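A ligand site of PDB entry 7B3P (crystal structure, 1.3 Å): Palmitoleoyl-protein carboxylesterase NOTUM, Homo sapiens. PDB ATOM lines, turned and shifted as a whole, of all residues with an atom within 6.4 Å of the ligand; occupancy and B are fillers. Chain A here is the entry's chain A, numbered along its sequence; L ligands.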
ATOM      1  N   GLY A  49      -0.105 -19.942   2.869  1.00  0.00           N
ATOM      2  CA  GLY A  49      -1.266 -19.552   2.110  1.00  0.00           C
ATOM      3  C   GLY A  49      -1.703 -18.117   2.373  1.00  0.00           C
ATOM      4  O   GLY A  49      -0.972 -17.296   2.933  1.00  0.00           O
ATOM      5  N   GLY A  50      -2.924 -17.800   1.918  1.00  0.00           N
ATOM      6  CA  GLY A  50      -3.446 -16.456   2.022  1.00  0.00           C
ATOM      7  C   GLY A  50      -4.127 -15.900   0.778  1.00  0.00           C
ATOM      8  O   GLY A  50      -3.861 -14.758   0.394  1.00  0.00           O
ATOM      9  N   TRP A  51      -5.016 -16.663   0.157  1.00  0.00           N
ATOM     10  CA  TRP A  51      -5.820 -16.218  -0.991  1.00  0.00           C
ATOM     11  C   TRP A  51      -4.901 -15.761  -2.124  1.00  0.00           C
ATOM     12  O   TRP A  51      -3.906 -16.444  -2.405  1.00  0.00           O
ATOM     13  CB  TRP A  51      -6.954 -15.297  -0.606  1.00  0.00           C
ATOM     14  CG  TRP A  51      -7.952 -15.988   0.258  1.00  0.00           C
ATOM     15  CD1 TRP A  51      -8.019 -15.983   1.612  1.00  0.00           C
ATOM     16  CD2 TRP A  51      -9.026 -16.830  -0.201  1.00  0.00           C
ATOM     17  NE1 TRP A  51      -9.092 -16.743   2.040  1.00  0.00           N
ATOM     18  CE2 TRP A  51      -9.712 -17.282   0.943  1.00  0.00           C
ATOM     19  CE3 TRP A  51      -9.451 -17.248  -1.457  1.00  0.00           C
ATOM     20  CZ2 TRP A  51     -10.830 -18.115   0.866  1.00  0.00           C
ATOM     21  CZ3 TRP A  51     -10.561 -18.077  -1.544  1.00  0.00           C
ATOM     22  CH2 TRP A  51     -11.235 -18.505  -0.373  1.00  0.00           C
ATOM     23  N   TYR A  52      -5.221 -14.663  -2.799  1.00  0.00           N
ATOM     24  CA  TYR A  52      -4.555 -14.185  -3.998  1.00  0.00           C
ATOM     25  C   TYR A  52      -5.213 -12.855  -4.349  1.00  0.00           C
ATOM     26  O   TYR A  52      -6.215 -12.482  -3.738  1.00  0.00           O
ATOM     27  CB  TYR A  52      -4.661 -15.185  -5.152  1.00  0.00           C
ATOM     28  CG  TYR A  52      -6.064 -15.527  -5.590  1.00  0.00           C
ATOM     29  CD1 TYR A  52      -6.763 -16.547  -4.976  1.00  0.00           C
ATOM     30  CD2 TYR A  52      -6.674 -14.849  -6.640  1.00  0.00           C
ATOM     31  CE1 TYR A  52      -8.064 -16.876  -5.364  1.00  0.00           C
ATOM     32  CE2 TYR A  52      -7.969 -15.192  -7.065  1.00  0.00           C
ATOM     33  CZ  TYR A  52      -8.641 -16.213  -6.411  1.00  0.00           C
ATOM     34  OH  TYR A  52      -9.928 -16.547  -6.808  1.00  0.00           O
ATOM     35  N   TYR A 105       4.429 -16.352   1.710  1.00  0.00           N
ATOM     36  CA  TYR A 105       3.644 -16.118   0.504  1.00  0.00           C
ATOM     37  C   TYR A 105       3.536 -14.610   0.304  1.00  0.00           C
ATOM     38  O   TYR A 105       2.842 -13.915   1.051  1.00  0.00           O
ATOM     39  CB  TYR A 105       2.278 -16.741   0.706  1.00  0.00           C
ATOM     40  CG  TYR A 105       1.291 -16.608  -0.416  1.00  0.00           C
ATOM     41  CD1 TYR A 105       1.663 -16.800  -1.749  1.00  0.00           C
ATOM     42  CD2 TYR A 105      -0.055 -16.408  -0.136  1.00  0.00           C
ATOM     43  CE1 TYR A 105       0.708 -16.764  -2.775  1.00  0.00           C
ATOM     44  CE2 TYR A 105      -1.002 -16.361  -1.124  1.00  0.00           C
ATOM     45  CZ  TYR A 105      -0.606 -16.536  -2.449  1.00  0.00           C
ATOM     46  OH  TYR A 105      -1.533 -16.504  -3.464  1.00  0.00           O
ATOM     47  N   VAL A 110      -1.132 -17.713  -5.998  1.00  0.00           N
ATOM     48  CA  VAL A 110      -1.278 -19.137  -5.682  1.00  0.00           C
ATOM     49  C   VAL A 110       0.014 -19.876  -6.072  1.00  0.00           C
ATOM     50  O   VAL A 110      -0.005 -21.051  -6.491  1.00  0.00           O
ATOM     51  CB  VAL A 110      -2.550 -19.738  -6.321  1.00  0.00           C
ATOM     52  CG1 VAL A 110      -2.849 -21.107  -5.731  1.00  0.00           C
ATOM     53  CG2 VAL A 110      -3.744 -18.813  -6.200  1.00  0.00           C
ATOM     54  N   SER A 154      -0.207 -24.986   2.865  1.00  0.00           N
ATOM     55  CA  SER A 154      -1.596 -24.906   3.305  1.00  0.00           C
ATOM     56  C   SER A 154      -2.361 -23.845   2.509  1.00  0.00           C
ATOM     57  O   SER A 154      -1.849 -22.741   2.255  1.00  0.00           O
ATOM     58  CB  SER A 154      -1.724 -24.573   4.790  1.00  0.00           C
ATOM     59  OG  SER A 154      -1.133 -25.597   5.609  1.00  0.00           O
ATOM     60  N   SER A 155      -3.616 -24.185   2.174  1.00  0.00           N
ATOM     61  CA  SER A 155      -4.580 -23.301   1.494  1.00  0.00           C
ATOM     62  C   SER A 155      -3.998 -22.901   0.134  1.00  0.00           C
ATOM     63  O   SER A 155      -3.762 -23.800  -0.688  1.00  0.00           O
ATOM     64  CB  SER A 155      -5.158 -22.200   2.393  1.00  0.00           C
ATOM     65  OG  SER A 155      -4.319 -21.062   2.491  1.00  0.00           O
ATOM     66  N   ALA A 156      -3.768 -21.610  -0.151  1.00  0.00           N
ATOM     67  CA  ALA A 156      -3.108 -21.265  -1.411  1.00  0.00           C
ATOM     68  C   ALA A 156      -1.775 -21.997  -1.539  1.00  0.00           C
ATOM     69  O   ALA A 156      -1.372 -22.327  -2.659  1.00  0.00           O
ATOM     70  CB  ALA A 156      -2.898 -19.743  -1.509  1.00  0.00           C
ATOM     71  N   GLY A 157      -1.089 -22.234  -0.414  1.00  0.00           N
ATOM     72  CA  GLY A 157       0.150 -23.010  -0.446  1.00  0.00           C
ATOM     73  C   GLY A 157      -0.066 -24.481  -0.750  1.00  0.00           C
ATOM     74  O   GLY A 157       0.804 -25.134  -1.330  1.00  0.00           O
ATOM     75  N   THR A 159      -2.549 -25.660  -2.801  1.00  0.00           N
ATOM     76  CA  THR A 159      -2.639 -25.673  -4.256  1.00  0.00           C
ATOM     77  C   THR A 159      -1.264 -25.408  -4.870  1.00  0.00           C
ATOM     78  O   THR A 159      -0.897 -26.027  -5.875  1.00  0.00           O
ATOM     79  CB  THR A 159      -3.670 -24.632  -4.728  1.00  0.00           C
ATOM     80  OG1 THR A 159      -4.886 -24.812  -3.985  1.00  0.00           O
ATOM     81  CG2 THR A 159      -3.916 -24.758  -6.209  1.00  0.00           C
ATOM     82  N   SER A 188      -5.394 -28.520   2.532  1.00  0.00           N
ATOM     83  CA  SER A 188      -6.460 -27.531   2.391  1.00  0.00           C
ATOM     84  C   SER A 188      -6.375 -26.756   1.081  1.00  0.00           C
ATOM     85  O   SER A 188      -6.762 -25.581   1.009  1.00  0.00           O
ATOM     86  CB  SER A 188      -6.482 -26.602   3.605  1.00  0.00           C
ATOM     87  OG  SER A 188      -6.671 -27.377   4.803  1.00  0.00           O
ATOM     88  N   GLY A 189      -5.896 -27.429   0.045  1.00  0.00           N
ATOM     89  CA  GLY A 189      -5.772 -26.832  -1.269  1.00  0.00           C
ATOM     90  C   GLY A 189      -6.498 -27.579  -2.356  1.00  0.00           C
ATOM     91  O   GLY A 189      -6.204 -27.356  -3.540  1.00  0.00           O
ATOM     92  N   PHE A 191      -9.941 -28.253  -4.028  1.00  0.00           N
ATOM     93  CA  PHE A 191     -11.252 -27.623  -4.106  1.00  0.00           C
ATOM     94  C   PHE A 191     -12.096 -28.222  -5.227  1.00  0.00           C
ATOM     95  O   PHE A 191     -11.574 -28.853  -6.158  1.00  0.00           O
ATOM     96  CB  PHE A 191     -11.105 -26.112  -4.324  1.00  0.00           C
ATOM     97  CG  PHE A 191     -10.351 -25.465  -3.221  1.00  0.00           C
ATOM     98  CD1 PHE A 191     -10.896 -25.440  -1.956  1.00  0.00           C
ATOM     99  CD2 PHE A 191      -9.076 -24.981  -3.414  1.00  0.00           C
ATOM    100  CE1 PHE A 191     -10.177 -24.917  -0.906  1.00  0.00           C
ATOM    101  CE2 PHE A 191      -8.375 -24.447  -2.365  1.00  0.00           C
ATOM    102  CZ  PHE A 191      -8.909 -24.406  -1.122  1.00  0.00           C
ATOM    103  N   PRO A 210     -14.533 -18.393  -8.192  1.00  0.00           N
ATOM    104  CA  PRO A 210     -13.105 -18.737  -8.277  1.00  0.00           C
ATOM    105  C   PRO A 210     -12.635 -19.023  -9.685  1.00  0.00           C
ATOM    106  O   PRO A 210     -11.550 -18.582 -10.075  1.00  0.00           O
ATOM    107  CB  PRO A 210     -13.008 -20.004  -7.406  1.00  0.00           C
ATOM    108  CG  PRO A 210     -14.097 -19.837  -6.400  1.00  0.00           C
ATOM    109  CD  PRO A 210     -15.223 -19.093  -7.091  1.00  0.00           C
ATOM    110  N   ILE A 214      -9.764 -16.942 -10.853  1.00  0.00           N
ATOM    111  CA  ILE A 214      -8.526 -17.627 -11.212  1.00  0.00           C
ATOM    112  C   ILE A 214      -8.173 -17.423 -12.676  1.00  0.00           C
ATOM    113  O   ILE A 214      -7.010 -17.200 -13.022  1.00  0.00           O
ATOM    114  CB  ILE A 214      -8.562 -19.123 -10.813  1.00  0.00           C
ATOM    115  CG1 ILE A 214      -8.528 -19.280  -9.302  1.00  0.00           C
ATOM    116  CG2 ILE A 214      -7.411 -19.896 -11.453  1.00  0.00           C
ATOM    117  CD1 ILE A 214      -7.246 -18.733  -8.675  1.00  0.00           C
ATOM    118  N   TRP A 239      -6.813 -22.742 -15.931  1.00  0.00           N
ATOM    119  CA  TRP A 239      -7.479 -22.669 -14.633  1.00  0.00           C
ATOM    120  C   TRP A 239      -7.877 -24.038 -14.106  1.00  0.00           C
ATOM    121  O   TRP A 239      -7.962 -24.233 -12.893  1.00  0.00           O
ATOM    122  CB  TRP A 239      -8.714 -21.743 -14.726  1.00  0.00           C
ATOM    123  CG  TRP A 239      -9.835 -22.298 -15.593  1.00  0.00           C
ATOM    124  CD1 TRP A 239     -10.048 -22.034 -16.920  1.00  0.00           C
ATOM    125  CD2 TRP A 239     -10.871 -23.219 -15.200  1.00  0.00           C
ATOM    126  NE1 TRP A 239     -11.149 -22.735 -17.361  1.00  0.00           N
ATOM    127  CE2 TRP A 239     -11.656 -23.474 -16.333  1.00  0.00           C
ATOM    128  CE3 TRP A 239     -11.170 -23.874 -14.011  1.00  0.00           C
ATOM    129  CZ2 TRP A 239     -12.775 -24.350 -16.302  1.00  0.00           C
ATOM    130  CZ3 TRP A 239     -12.275 -24.751 -13.970  1.00  0.00           C
ATOM    131  CH2 TRP A 239     -13.045 -24.974 -15.107  1.00  0.00           C
ATOM    132  N   PHE A 242      -5.762 -25.677 -11.398  1.00  0.00           N
ATOM    133  CA  PHE A 242      -5.801 -25.234 -10.019  1.00  0.00           C
ATOM    134  C   PHE A 242      -6.720 -26.093  -9.169  1.00  0.00           C
ATOM    135  O   PHE A 242      -6.758 -25.924  -7.951  1.00  0.00           O
ATOM    136  CB  PHE A 242      -6.242 -23.761  -9.954  1.00  0.00           C
ATOM    137  CG  PHE A 242      -5.138 -22.782 -10.254  1.00  0.00           C
ATOM    138  CD1 PHE A 242      -4.515 -22.778 -11.492  1.00  0.00           C
ATOM    139  CD2 PHE A 242      -4.813 -21.789  -9.329  1.00  0.00           C
ATOM    140  CE1 PHE A 242      -3.502 -21.842 -11.776  1.00  0.00           C
ATOM    141  CE2 PHE A 242      -3.827 -20.849  -9.634  1.00  0.00           C
ATOM    142  CZ  PHE A 242      -3.172 -20.889 -10.825  1.00  0.00           C
ATOM    143  N   PHE A 243      -7.470 -27.008  -9.796  1.00  0.00           N
ATOM    144  CA  PHE A 243      -8.388 -27.886  -9.075  1.00  0.00           C
ATOM    145  C   PHE A 243      -7.703 -29.223  -8.875  1.00  0.00           C
ATOM    146  O   PHE A 243      -7.374 -29.910  -9.850  1.00  0.00           O
ATOM    147  CB  PHE A 243      -9.722 -27.958  -9.806  1.00  0.00           C
ATOM    148  CG  PHE A 243     -10.481 -26.686  -9.673  1.00  0.00           C
ATOM    149  CD1 PHE A 243     -11.315 -26.503  -8.596  1.00  0.00           C
ATOM    150  CD2 PHE A 243     -10.241 -25.622 -10.530  1.00  0.00           C
ATOM    151  CE1 PHE A 243     -11.970 -25.276  -8.405  1.00  0.00           C
ATOM    152  CE2 PHE A 243     -10.877 -24.404 -10.317  1.00  0.00           C
ATOM    153  CZ  PHE A 243     -11.754 -24.252  -9.266  1.00  0.00           C
ATOM    154  N   ASP A 263     -14.541 -28.082   4.003  1.00  0.00           N
ATOM    155  CA  ASP A 263     -13.580 -27.000   4.172  1.00  0.00           C
ATOM    156  C   ASP A 263     -14.301 -25.649   4.202  1.00  0.00           C
ATOM    157  O   ASP A 263     -15.157 -25.366   3.362  1.00  0.00           O
ATOM    158  CB  ASP A 263     -12.594 -27.079   3.000  1.00  0.00           C
ATOM    159  CG  ASP A 263     -11.528 -26.064   3.079  1.00  0.00           C
ATOM    160  OD1 ASP A 263     -10.505 -26.320   3.725  1.00  0.00           O
ATOM    161  OD2 ASP A 263     -11.757 -24.963   2.515  1.00  0.00           O
ATOM    162  N   ALA A 265     -13.281 -22.661   3.455  1.00  0.00           N
ATOM    163  CA  ALA A 265     -13.098 -21.813   2.296  1.00  0.00           C
ATOM    164  C   ALA A 265     -13.954 -22.283   1.135  1.00  0.00           C
ATOM    165  O   ALA A 265     -14.522 -21.458   0.397  1.00  0.00           O
ATOM    166  CB  ALA A 265     -11.630 -21.731   1.883  1.00  0.00           C
ATOM    167  N   GLN A 266     -14.070 -23.609   0.971  1.00  0.00           N
ATOM    168  CA  GLN A 266     -14.981 -24.159  -0.026  1.00  0.00           C
ATOM    169  C   GLN A 266     -16.410 -23.690   0.252  1.00  0.00           C
ATOM    170  O   GLN A 266     -17.089 -23.187  -0.650  1.00  0.00           O
ATOM    171  CB  GLN A 266     -14.898 -25.689  -0.006  1.00  0.00           C
ATOM    172  CG  GLN A 266     -15.838 -26.362  -0.985  1.00  0.00           C
ATOM    173  CD  GLN A 266     -15.330 -26.328  -2.411  1.00  0.00           C
ATOM    174  OE1 GLN A 266     -14.183 -26.700  -2.687  1.00  0.00           O
ATOM    175  NE2 GLN A 266     -16.182 -25.890  -3.336  1.00  0.00           N
ATOM    176  N   HIS A 312     -11.335 -24.479   9.020  1.00  0.00           N
ATOM    177  CA  HIS A 312     -10.271 -23.824   8.264  1.00  0.00           C
ATOM    178  C   HIS A 312      -8.898 -24.082   8.863  1.00  0.00           C
ATOM    179  O   HIS A 312      -7.936 -23.422   8.469  1.00  0.00           O
ATOM    180  CB  HIS A 312     -10.491 -22.312   8.153  1.00  0.00           C
ATOM    181  CG  HIS A 312     -10.511 -21.602   9.481  1.00  0.00           C
ATOM    182  ND1 HIS A 312     -11.656 -21.043  10.023  1.00  0.00           N
ATOM    183  CD2 HIS A 312      -9.514 -21.361  10.365  1.00  0.00           C
ATOM    184  CE1 HIS A 312     -11.356 -20.492  11.186  1.00  0.00           C
ATOM    185  NE2 HIS A 312     -10.072 -20.674  11.418  1.00  0.00           N
HETATM  186  C1  LIG L   1      -8.333 -22.275  -5.891  1.00  0.00           C
HETATM  187  C2  LIG L   1      -8.912 -21.087  -5.501  1.00  0.00           C
HETATM  188  C3  LIG L   1      -8.259 -20.334  -4.537  1.00  0.00           C
HETATM  189  C4  LIG L   1      -7.051 -20.796  -4.040  1.00  0.00           C
HETATM  190  C5  LIG L   1      -6.493 -22.008  -4.427  1.00  0.00           C
HETATM  191  C6  LIG L   1      -7.143 -22.745  -5.383  1.00  0.00           C
HETATM  192  C7  LIG L   1      -7.032 -20.105  -1.252  1.00  0.00           C
HETATM  193  C8  LIG L   1      -6.741 -19.098   2.300  1.00  0.00           C
HETATM  194  C9  LIG L   1      -8.209 -20.480   1.191  1.00  0.00           C
HETATM  195  C10 LIG L   1      -8.713 -21.149   0.094  1.00  0.00           C
HETATM  196  C11 LIG L   1      -8.154 -20.985  -1.160  1.00  0.00           C
HETATM  197  N1  LIG L   1      -6.562 -19.498  -0.186  1.00  0.00           N
HETATM  198  N2  LIG L   1      -7.119 -19.689   1.041  1.00  0.00           N
HETATM  199  N3  LIG L   1      -7.634 -19.601   3.268  1.00  0.00           N
HETATM  200  N4  LIG L   1      -8.537 -20.460   2.621  1.00  0.00           N
HETATM  201  O1  LIG L   1      -5.832 -18.339   2.437  1.00  0.00           O
HETATM  202  S1  LIG L   1      -6.212 -19.812  -2.806  1.00  0.00           S
HETATM  203 CL1  LIG L   1      -9.179 -23.246  -7.098  1.00  0.00          CL
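Residues that only touch the ligand: Tyr 52 (3.6 Å), Val 110 (3.97 Å), Ala 156 (3.5 Å), Thr 159 (3.3 Å), Phe 191 (3.5 Å), Phe 242 (3.7 Å), Phe 243 (3.5 Å) and Ala 265 (3.4 Å).
Hydrophobic or aromatic side chains within 4 Å of the ligand: Trp 51, Tyr 52, Val 110, Ala 156, Phe 191, Phe 243 and Ala 265.
Of the 23 residues printed, 11 come within 4 Å of the ligand.
Along chain A the residues within 4 Å of the ligand span positions 50 to 265.
The nearest printed residue that does not touch the ligand is Gly 49 (4.1 Å).
OH of Tyr 105 lies within hydrogen-bond range of O of Trp 51, 2.6 Å away.
The backbone carbonyl oxygen (O) of Gly 189 sits at hydrogen-bond distance from the side-chain hydroxyl (OG1) of Thr 159, at 2.9 Å.
N of Ala 265 lies within hydrogen-bond range of OD2 of Asp 263, at 2.9 Å.
The backbone NH of Val 110 sits at hydrogen-bond distance from the side-chain hydroxyl of Tyr 105 (2.8 Å).
The backbone NH (N) of Trp 51 sits at hydrogen-bond distance from an oxygen (O1) of the ligand (2.9 Å).
The backbone NH (N) of Gly 50 is in hydrogen-bond range of an oxygen (O1) of the ligand, at 3.0 Å.
The side-chain hydroxyl (OG) of Ser 155 lies within hydrogen-bond range of an oxygen (O1) of the ligand (3.1 Å).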
